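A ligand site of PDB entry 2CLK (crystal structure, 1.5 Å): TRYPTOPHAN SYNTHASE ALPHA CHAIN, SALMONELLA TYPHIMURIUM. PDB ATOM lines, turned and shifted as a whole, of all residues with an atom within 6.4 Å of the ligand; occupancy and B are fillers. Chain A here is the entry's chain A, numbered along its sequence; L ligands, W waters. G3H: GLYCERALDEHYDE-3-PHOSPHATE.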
ATOM      1  N   PHE A  22     -16.803  21.667  14.807  1.00  0.00           N
ATOM      2  CA  PHE A  22     -17.973  21.290  15.588  1.00  0.00           C
ATOM      3  C   PHE A  22     -17.629  21.214  17.090  1.00  0.00           C
ATOM      4  O   PHE A  22     -16.564  20.685  17.459  1.00  0.00           O
ATOM      5  CB  PHE A  22     -18.483  19.939  15.126  1.00  0.00           C
ATOM      6  CG  PHE A  22     -19.489  19.345  16.076  1.00  0.00           C
ATOM      7  CD1 PHE A  22     -19.095  18.622  17.203  1.00  0.00           C
ATOM      8  CD2 PHE A  22     -20.855  19.541  15.861  1.00  0.00           C
ATOM      9  CE1 PHE A  22     -20.084  18.072  18.085  1.00  0.00           C
ATOM     10  CE2 PHE A  22     -21.829  19.018  16.688  1.00  0.00           C
ATOM     11  CZ  PHE A  22     -21.480  18.312  17.800  1.00  0.00           C
ATOM     12  N   GLU A  49     -20.448  24.589  13.566  1.00  0.00           N
ATOM     13  CA  GLU A  49     -21.451  23.508  13.550  1.00  0.00           C
ATOM     14  C   GLU A  49     -21.577  23.210  15.060  1.00  0.00           C
ATOM     15  O   GLU A  49     -20.535  22.970  15.713  1.00  0.00           O
ATOM     16  CB  GLU A  49     -20.898  22.300  12.827  1.00  0.00           C
ATOM     17  CG  GLU A  49     -22.031  21.340  12.597  1.00  0.00           C
ATOM     18  CD  GLU A  49     -22.404  21.478  11.128  1.00  0.00           C
ATOM     19  OE1 GLU A  49     -22.162  22.590  10.613  1.00  0.00           O
ATOM     20  OE2 GLU A  49     -22.935  20.565  10.495  1.00  0.00           O
ATOM     21  N   ASP A  60     -23.114   9.348  16.803  1.00  0.00           N
ATOM     22  CA  ASP A  60     -21.821   9.772  17.356  1.00  0.00           C
ATOM     23  C   ASP A  60     -20.951   8.684  17.962  1.00  0.00           C
ATOM     24  O   ASP A  60     -21.447   7.839  18.696  1.00  0.00           O
ATOM     25  CB  ASP A  60     -22.033  10.903  18.419  1.00  0.00           C
ATOM     26  CG  ASP A  60     -22.388  12.207  17.771  1.00  0.00           C
ATOM     27  OD1 ASP A  60     -21.542  12.763  17.005  1.00  0.00           O
ATOM     28  OD2 ASP A  60     -23.498  12.775  18.085  1.00  0.00           O
ATOM     29  N   ILE A  64     -17.725  12.192  20.973  1.00  0.00           N
ATOM     30  CA  ILE A  64     -18.877  13.064  21.123  1.00  0.00           C
ATOM     31  C   ILE A  64     -19.897  12.493  22.156  1.00  0.00           C
ATOM     32  O   ILE A  64     -20.570  13.262  22.843  1.00  0.00           O
ATOM     33  CB  ILE A  64     -19.401  13.566  19.759  1.00  0.00           C
ATOM     34  CG1 ILE A  64     -18.323  14.544  19.202  1.00  0.00           C
ATOM     35  CG2 ILE A  64     -20.711  14.265  19.954  1.00  0.00           C
ATOM     36  CD1 ILE A  64     -18.483  14.764  17.763  1.00  0.00           C
ATOM     37  N   LEU A 100     -26.424  20.784  14.576  1.00  0.00           N
ATOM     38  CA  LEU A 100     -26.499  19.372  14.167  1.00  0.00           C
ATOM     39  C   LEU A 100     -27.318  18.783  15.313  1.00  0.00           C
ATOM     40  O   LEU A 100     -26.895  18.761  16.476  1.00  0.00           O
ATOM     41  CB  LEU A 100     -25.082  18.755  13.994  1.00  0.00           C
ATOM     42  CG  LEU A 100     -25.028  17.364  13.351  1.00  0.00           C
ATOM     43  CD1 LEU A 100     -23.599  17.017  12.902  1.00  0.00           C
ATOM     44  CD2 LEU A 100     -25.569  16.338  14.268  1.00  0.00           C
ATOM     45  N   LEU A 127     -29.070  20.595  10.536  1.00  0.00           N
ATOM     46  CA  LEU A 127     -28.982  19.208  10.077  1.00  0.00           C
ATOM     47  C   LEU A 127     -29.592  18.335  11.135  1.00  0.00           C
ATOM     48  O   LEU A 127     -29.200  18.388  12.268  1.00  0.00           O
ATOM     49  CB  LEU A 127     -27.509  18.768   9.912  1.00  0.00           C
ATOM     50  CG  LEU A 127     -27.321  17.251   9.641  1.00  0.00           C
ATOM     51  CD1 LEU A 127     -28.089  16.690   8.440  1.00  0.00           C
ATOM     52  CD2 LEU A 127     -25.777  16.953   9.451  1.00  0.00           C
ATOM     53  N   TYR A 175     -23.892  18.342   3.367  1.00  0.00           N
ATOM     54  CA  TYR A 175     -22.933  17.672   4.275  1.00  0.00           C
ATOM     55  C   TYR A 175     -22.455  16.430   3.578  1.00  0.00           C
ATOM     56  O   TYR A 175     -23.206  15.464   3.485  1.00  0.00           O
ATOM     57  CB  TYR A 175     -23.642  17.355   5.602  1.00  0.00           C
ATOM     58  CG  TYR A 175     -22.700  17.019   6.748  1.00  0.00           C
ATOM     59  CD1 TYR A 175     -21.873  15.956   6.638  1.00  0.00           C
ATOM     60  CD2 TYR A 175     -22.737  17.755   7.943  1.00  0.00           C
ATOM     61  CE1 TYR A 175     -20.989  15.590   7.679  1.00  0.00           C
ATOM     62  CE2 TYR A 175     -21.881  17.420   8.976  1.00  0.00           C
ATOM     63  CZ  TYR A 175     -21.005  16.346   8.816  1.00  0.00           C
ATOM     64  OH  TYR A 175     -20.136  15.946   9.819  1.00  0.00           O
ATOM     65  N   ARG A 179     -17.311   8.990   4.977  1.00  0.00           N
ATOM     66  CA  ARG A 179     -17.366   7.529   5.105  1.00  0.00           C
ATOM     67  C   ARG A 179     -18.610   7.077   5.848  1.00  0.00           C
ATOM     68  O   ARG A 179     -19.383   7.871   6.377  1.00  0.00           O
ATOM     69  CB  ARG A 179     -16.153   7.075   5.934  1.00  0.00           C
ATOM     70  CG  ARG A 179     -16.063   7.818   7.317  1.00  0.00           C
ATOM     71  CD  ARG A 179     -15.200   7.081   8.370  1.00  0.00           C
ATOM     72  NE  ARG A 179     -14.981   7.855   9.600  1.00  0.00           N
ATOM     73  CZ  ARG A 179     -15.879   8.002  10.554  1.00  0.00           C
ATOM     74  NH1 ARG A 179     -17.073   7.416  10.450  1.00  0.00           N
ATOM     75  NH2 ARG A 179     -15.564   8.737  11.625  1.00  0.00           N
ATOM     76  N   VAL A 182     -19.871   6.278  12.355  1.00  0.00           N
ATOM     77  CA  VAL A 182     -20.326   7.371  13.189  1.00  0.00           C
ATOM     78  C   VAL A 182     -19.193   8.383  13.376  1.00  0.00           C
ATOM     79  O   VAL A 182     -18.060   8.111  12.961  1.00  0.00           O
ATOM     80  CB  VAL A 182     -20.756   6.880  14.592  1.00  0.00           C
ATOM     81  CG1 VAL A 182     -22.030   6.058  14.459  1.00  0.00           C
ATOM     82  CG2 VAL A 182     -19.666   6.104  15.293  1.00  0.00           C
ATOM     83  N   THR A 183     -19.464   9.508  14.036  1.00  0.00           N
ATOM     84  CA  THR A 183     -18.389  10.511  14.149  1.00  0.00           C
ATOM     85  C   THR A 183     -17.166   9.933  14.897  1.00  0.00           C
ATOM     86  O   THR A 183     -17.280   9.000  15.758  1.00  0.00           O
ATOM     87  CB  THR A 183     -18.899  11.776  14.860  1.00  0.00           C
ATOM     88  OG1 THR A 183     -19.304  11.467  16.183  1.00  0.00           O
ATOM     89  CG2 THR A 183     -20.106  12.409  14.124  1.00  0.00           C
ATOM     90  N   GLY A 184     -15.972  10.483  14.609  1.00  0.00           N
ATOM     91  CA  GLY A 184     -14.775  10.047  15.356  1.00  0.00           C
ATOM     92  C   GLY A 184     -13.549  10.385  14.551  1.00  0.00           C
ATOM     93  O   GLY A 184     -13.500  10.112  13.328  1.00  0.00           O
ATOM     94  N   ALA A 185     -12.568  10.953  15.256  1.00  0.00           N
ATOM     95  CA  ALA A 185     -11.328  11.407  14.671  1.00  0.00           C
ATOM     96  C   ALA A 185     -10.386  10.244  14.378  1.00  0.00           C
ATOM     97  O   ALA A 185      -9.510  10.377  13.512  1.00  0.00           O
ATOM     98  CB  ALA A 185     -10.648  12.447  15.606  1.00  0.00           C
ATOM     99  N   ASN A 187     -11.068   7.273  12.983  1.00  0.00           N
ATOM    100  CA  ASN A 187     -11.450   6.684  11.672  1.00  0.00           C
ATOM    101  C   ASN A 187     -11.525   7.668  10.473  1.00  0.00           C
ATOM    102  O   ASN A 187     -12.453   8.470  10.331  1.00  0.00           O
ATOM    103  CB  ASN A 187     -12.761   5.939  11.898  1.00  0.00           C
ATOM    104  CG  ASN A 187     -13.197   5.169  10.664  1.00  0.00           C
ATOM    105  OD1 ASN A 187     -12.540   5.217   9.631  1.00  0.00           O
ATOM    106  ND2 ASN A 187     -14.333   4.466  10.761  1.00  0.00           N
ATOM    107  N   GLY A 211     -17.387  16.098   5.936  1.00  0.00           N
ATOM    108  CA  GLY A 211     -17.303  15.845   7.386  1.00  0.00           C
ATOM    109  C   GLY A 211     -17.340  14.372   7.761  1.00  0.00           C
ATOM    110  O   GLY A 211     -17.894  13.567   6.987  1.00  0.00           O
ATOM    111  N   PHE A 212     -16.830  14.113   8.985  1.00  0.00           N
ATOM    112  CA  PHE A 212     -16.573  12.789   9.613  1.00  0.00           C
ATOM    113  C   PHE A 212     -15.104  12.416   9.385  1.00  0.00           C
ATOM    114  O   PHE A 212     -14.638  12.288   8.215  1.00  0.00           O
ATOM    115  CB  PHE A 212     -17.460  11.623   9.108  1.00  0.00           C
ATOM    116  CG  PHE A 212     -18.856  11.540   9.742  1.00  0.00           C
ATOM    117  CD1 PHE A 212     -19.601  12.670  10.017  1.00  0.00           C
ATOM    118  CD2 PHE A 212     -19.422  10.322   9.992  1.00  0.00           C
ATOM    119  CE1 PHE A 212     -20.895  12.593  10.562  1.00  0.00           C
ATOM    120  CE2 PHE A 212     -20.706  10.214  10.532  1.00  0.00           C
ATOM    121  CZ  PHE A 212     -21.437  11.339  10.826  1.00  0.00           C
ATOM    122  N   GLY A 213     -14.391  12.243  10.520  1.00  0.00           N
ATOM    123  CA  GLY A 213     -12.986  11.791  10.490  1.00  0.00           C
ATOM    124  C   GLY A 213     -11.931  12.862  10.097  1.00  0.00           C
ATOM    125  O   GLY A 213     -10.760  12.497   9.946  1.00  0.00           O
ATOM    126  N   ILE A 214     -12.289  14.134   9.883  1.00  0.00           N
ATOM    127  CA  ILE A 214     -11.326  15.159   9.437  1.00  0.00           C
ATOM    128  C   ILE A 214     -10.588  15.660  10.654  1.00  0.00           C
ATOM    129  O   ILE A 214     -11.198  16.379  11.514  1.00  0.00           O
ATOM    130  CB  ILE A 214     -12.077  16.360   8.767  1.00  0.00           C
ATOM    131  CG1 ILE A 214     -12.867  15.967   7.533  1.00  0.00           C
ATOM    132  CG2 ILE A 214     -11.079  17.490   8.432  1.00  0.00           C
ATOM    133  CD1 ILE A 214     -12.078  15.608   6.392  1.00  0.00           C
ATOM    134  N   SER A 215      -9.307  15.308  10.772  1.00  0.00           N
ATOM    135  CA  SER A 215      -8.579  15.653  11.957  1.00  0.00           C
ATOM    136  C   SER A 215      -7.185  16.258  11.712  1.00  0.00           C
ATOM    137  O   SER A 215      -6.449  16.496  12.667  1.00  0.00           O
ATOM    138  CB  SER A 215      -8.432  14.432  12.846  1.00  0.00           C
ATOM    139  OG  SER A 215      -7.651  13.435  12.140  1.00  0.00           O
ATOM    140  N   ILE A 232     -15.498  20.042   7.692  1.00  0.00           N
ATOM    141  CA  ILE A 232     -15.932  20.144   9.107  1.00  0.00           C
ATOM    142  C   ILE A 232     -15.100  19.187   9.956  1.00  0.00           C
ATOM    143  O   ILE A 232     -14.866  18.004   9.514  1.00  0.00           O
ATOM    144  CB  ILE A 232     -17.446  19.709   9.214  1.00  0.00           C
ATOM    145  CG1 ILE A 232     -18.289  20.729   8.467  1.00  0.00           C
ATOM    146  CG2 ILE A 232     -17.912  19.617  10.736  1.00  0.00           C
ATOM    147  CD1 ILE A 232     -19.774  20.114   8.140  1.00  0.00           C
ATOM    148  N   SER A 233     -14.719  19.664  11.144  1.00  0.00           N
ATOM    149  CA  SER A 233     -13.963  18.806  12.100  1.00  0.00           C
ATOM    150  C   SER A 233     -14.585  18.892  13.483  1.00  0.00           C
ATOM    151  O   SER A 233     -14.680  19.987  14.027  1.00  0.00           O
ATOM    152  CB  SER A 233     -12.527  19.311  12.218  1.00  0.00           C
ATOM    153  OG  SER A 233     -11.754  18.487  13.098  1.00  0.00           O
ATOM    154  N   GLY A 234     -15.007  17.764  14.058  1.00  0.00           N
ATOM    155  CA  GLY A 234     -15.657  17.870  15.353  1.00  0.00           C
ATOM    156  C   GLY A 234     -14.909  17.092  16.414  1.00  0.00           C
ATOM    157  O   GLY A 234     -14.373  17.687  17.364  1.00  0.00           O
ATOM    158  N   SER A 235     -14.849  15.751  16.250  1.00  0.00           N
ATOM    159  CA  SER A 235     -14.133  14.945  17.239  1.00  0.00           C
ATOM    160  C   SER A 235     -12.737  15.417  17.522  1.00  0.00           C
ATOM    161  O   SER A 235     -12.275  15.366  18.670  1.00  0.00           O
ATOM    162  CB  SER A 235     -14.104  13.444  16.793  1.00  0.00           C
ATOM    163  OG  SER A 235     -15.435  12.969  16.854  1.00  0.00           O
ATOM    164  N   ALA A 236     -12.028  15.833  16.495  1.00  0.00           N
ATOM    165  CA  ALA A 236     -10.675  16.343  16.737  1.00  0.00           C
ATOM    166  C   ALA A 236     -10.662  17.525  17.653  1.00  0.00           C
ATOM    167  O   ALA A 236      -9.770  17.627  18.510  1.00  0.00           O
ATOM    168  CB  ALA A 236      -9.969  16.662  15.454  1.00  0.00           C
HETATM  169  O1  G3H L   1     -20.318  17.514  12.017  1.00  0.00           O
HETATM  170  C1  G3H L   1     -19.946  17.041  13.179  1.00  0.00           C
HETATM  171  C2  G3H L   1     -19.227  15.749  13.259  1.00  0.00           C
HETATM  172  O2  G3H L   1     -18.877  15.770  14.672  1.00  0.00           O
HETATM  173  C3  G3H L   1     -17.945  15.718  12.414  1.00  0.00           C
HETATM  174  O1P G3H L   1     -17.351  14.406  12.369  1.00  0.00           O
HETATM  175  O2P G3H L   1     -15.040  15.170  13.014  1.00  0.00           O
HETATM  176  O3P G3H L   1     -15.742  12.688  12.866  1.00  0.00           O
HETATM  177  O4P G3H L   1     -16.571  14.174  14.772  1.00  0.00           O
HETATM  178  P   G3H L   1     -16.091  14.095  13.319  1.00  0.00           P
HETATM  179  O   HOH W   1     -21.707  15.284  15.968  1.00  0.00           O
HETATM  180  O   HOH W   2     -12.546  15.057  13.799  1.00  0.00           O
HETATM  181  O   HOH W   3     -14.835  15.390  10.346  1.00  0.00           O
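OG of Ser 235 lies close to N of Gly 184. The guanidinium group (NH2) of Arg 179 lies within hydrogen-bond range of the backbone carbonyl oxygen (O) of Gly 184. The side-chain hydroxyl (OG1) of Thr 183 lies within hydrogen-bond range of the side-chain carboxylate (OD1) of Asp 60 (2.7 Å). The backbone carbonyl oxygen (O) of Ser 233 lies within hydrogen-bond range of the backbone NH (N) of Phe 22, at 2.8 Å. The backbone carbonyl oxygen (O) of Ile 214 sits at hydrogen-bond distance from the side-chain hydroxyl (OG) of Ser 233 (2.7 Å).
Water W2 lies within hydrogen-bond range of an oxygen (O2P) of the ligand, the backbone NH of Ala 236, the backbone carbonyl oxygen of Ile 214 and the backbone NH of Ser 235. Water W1 lies within hydrogen-bond range of the side-chain carboxylate of Asp 60 (2.7 Å) and an oxygen (O2) of the ligand (3.2 Å).
N of Ser 235 lies within hydrogen-bond range of O4P of the ligand, 2.8 Å away. OG of Ser 235 lies within hydrogen-bond range of O4P of the ligand. The side-chain hydroxyl (OH) of Tyr 175 lies within hydrogen-bond range of an oxygen (O1) of the ligand (2.7 Å). O3P of the ligand sits at hydrogen-bond distance from N of Gly 213 (2.7 Å). O2P of the ligand sits at hydrogen-bond distance from N of Gly 234 (2.8 Å). The backbone NH (N) of Gly 184 sits at hydrogen-bond distance from an oxygen (O3P) of the ligand. The backbone NH (N) of Phe 212 lies close to an oxygen (O1P) of the ligand (3.4 Å).
Phe 22 touches the ligand (CG to C1, 3.7 Å). Ile 64 touches the ligand. CD1 of Leu 100 touches O1 of the ligand, 3.4 Å away. CB of Thr 183 touches O4P of the ligand, 3.3 Å away. CG2 of Ile 232 touches O1 of the ligand (3.4 Å). Ser 233 touches the ligand. Hydrophobic or aromatic side chains that line the ligand: Phe 22, Ile 64, Leu 100, Tyr 175, Phe 212 and Ile 232. The nearest printed residue that does not touch the ligand is Arg 179 (4.1 Å).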
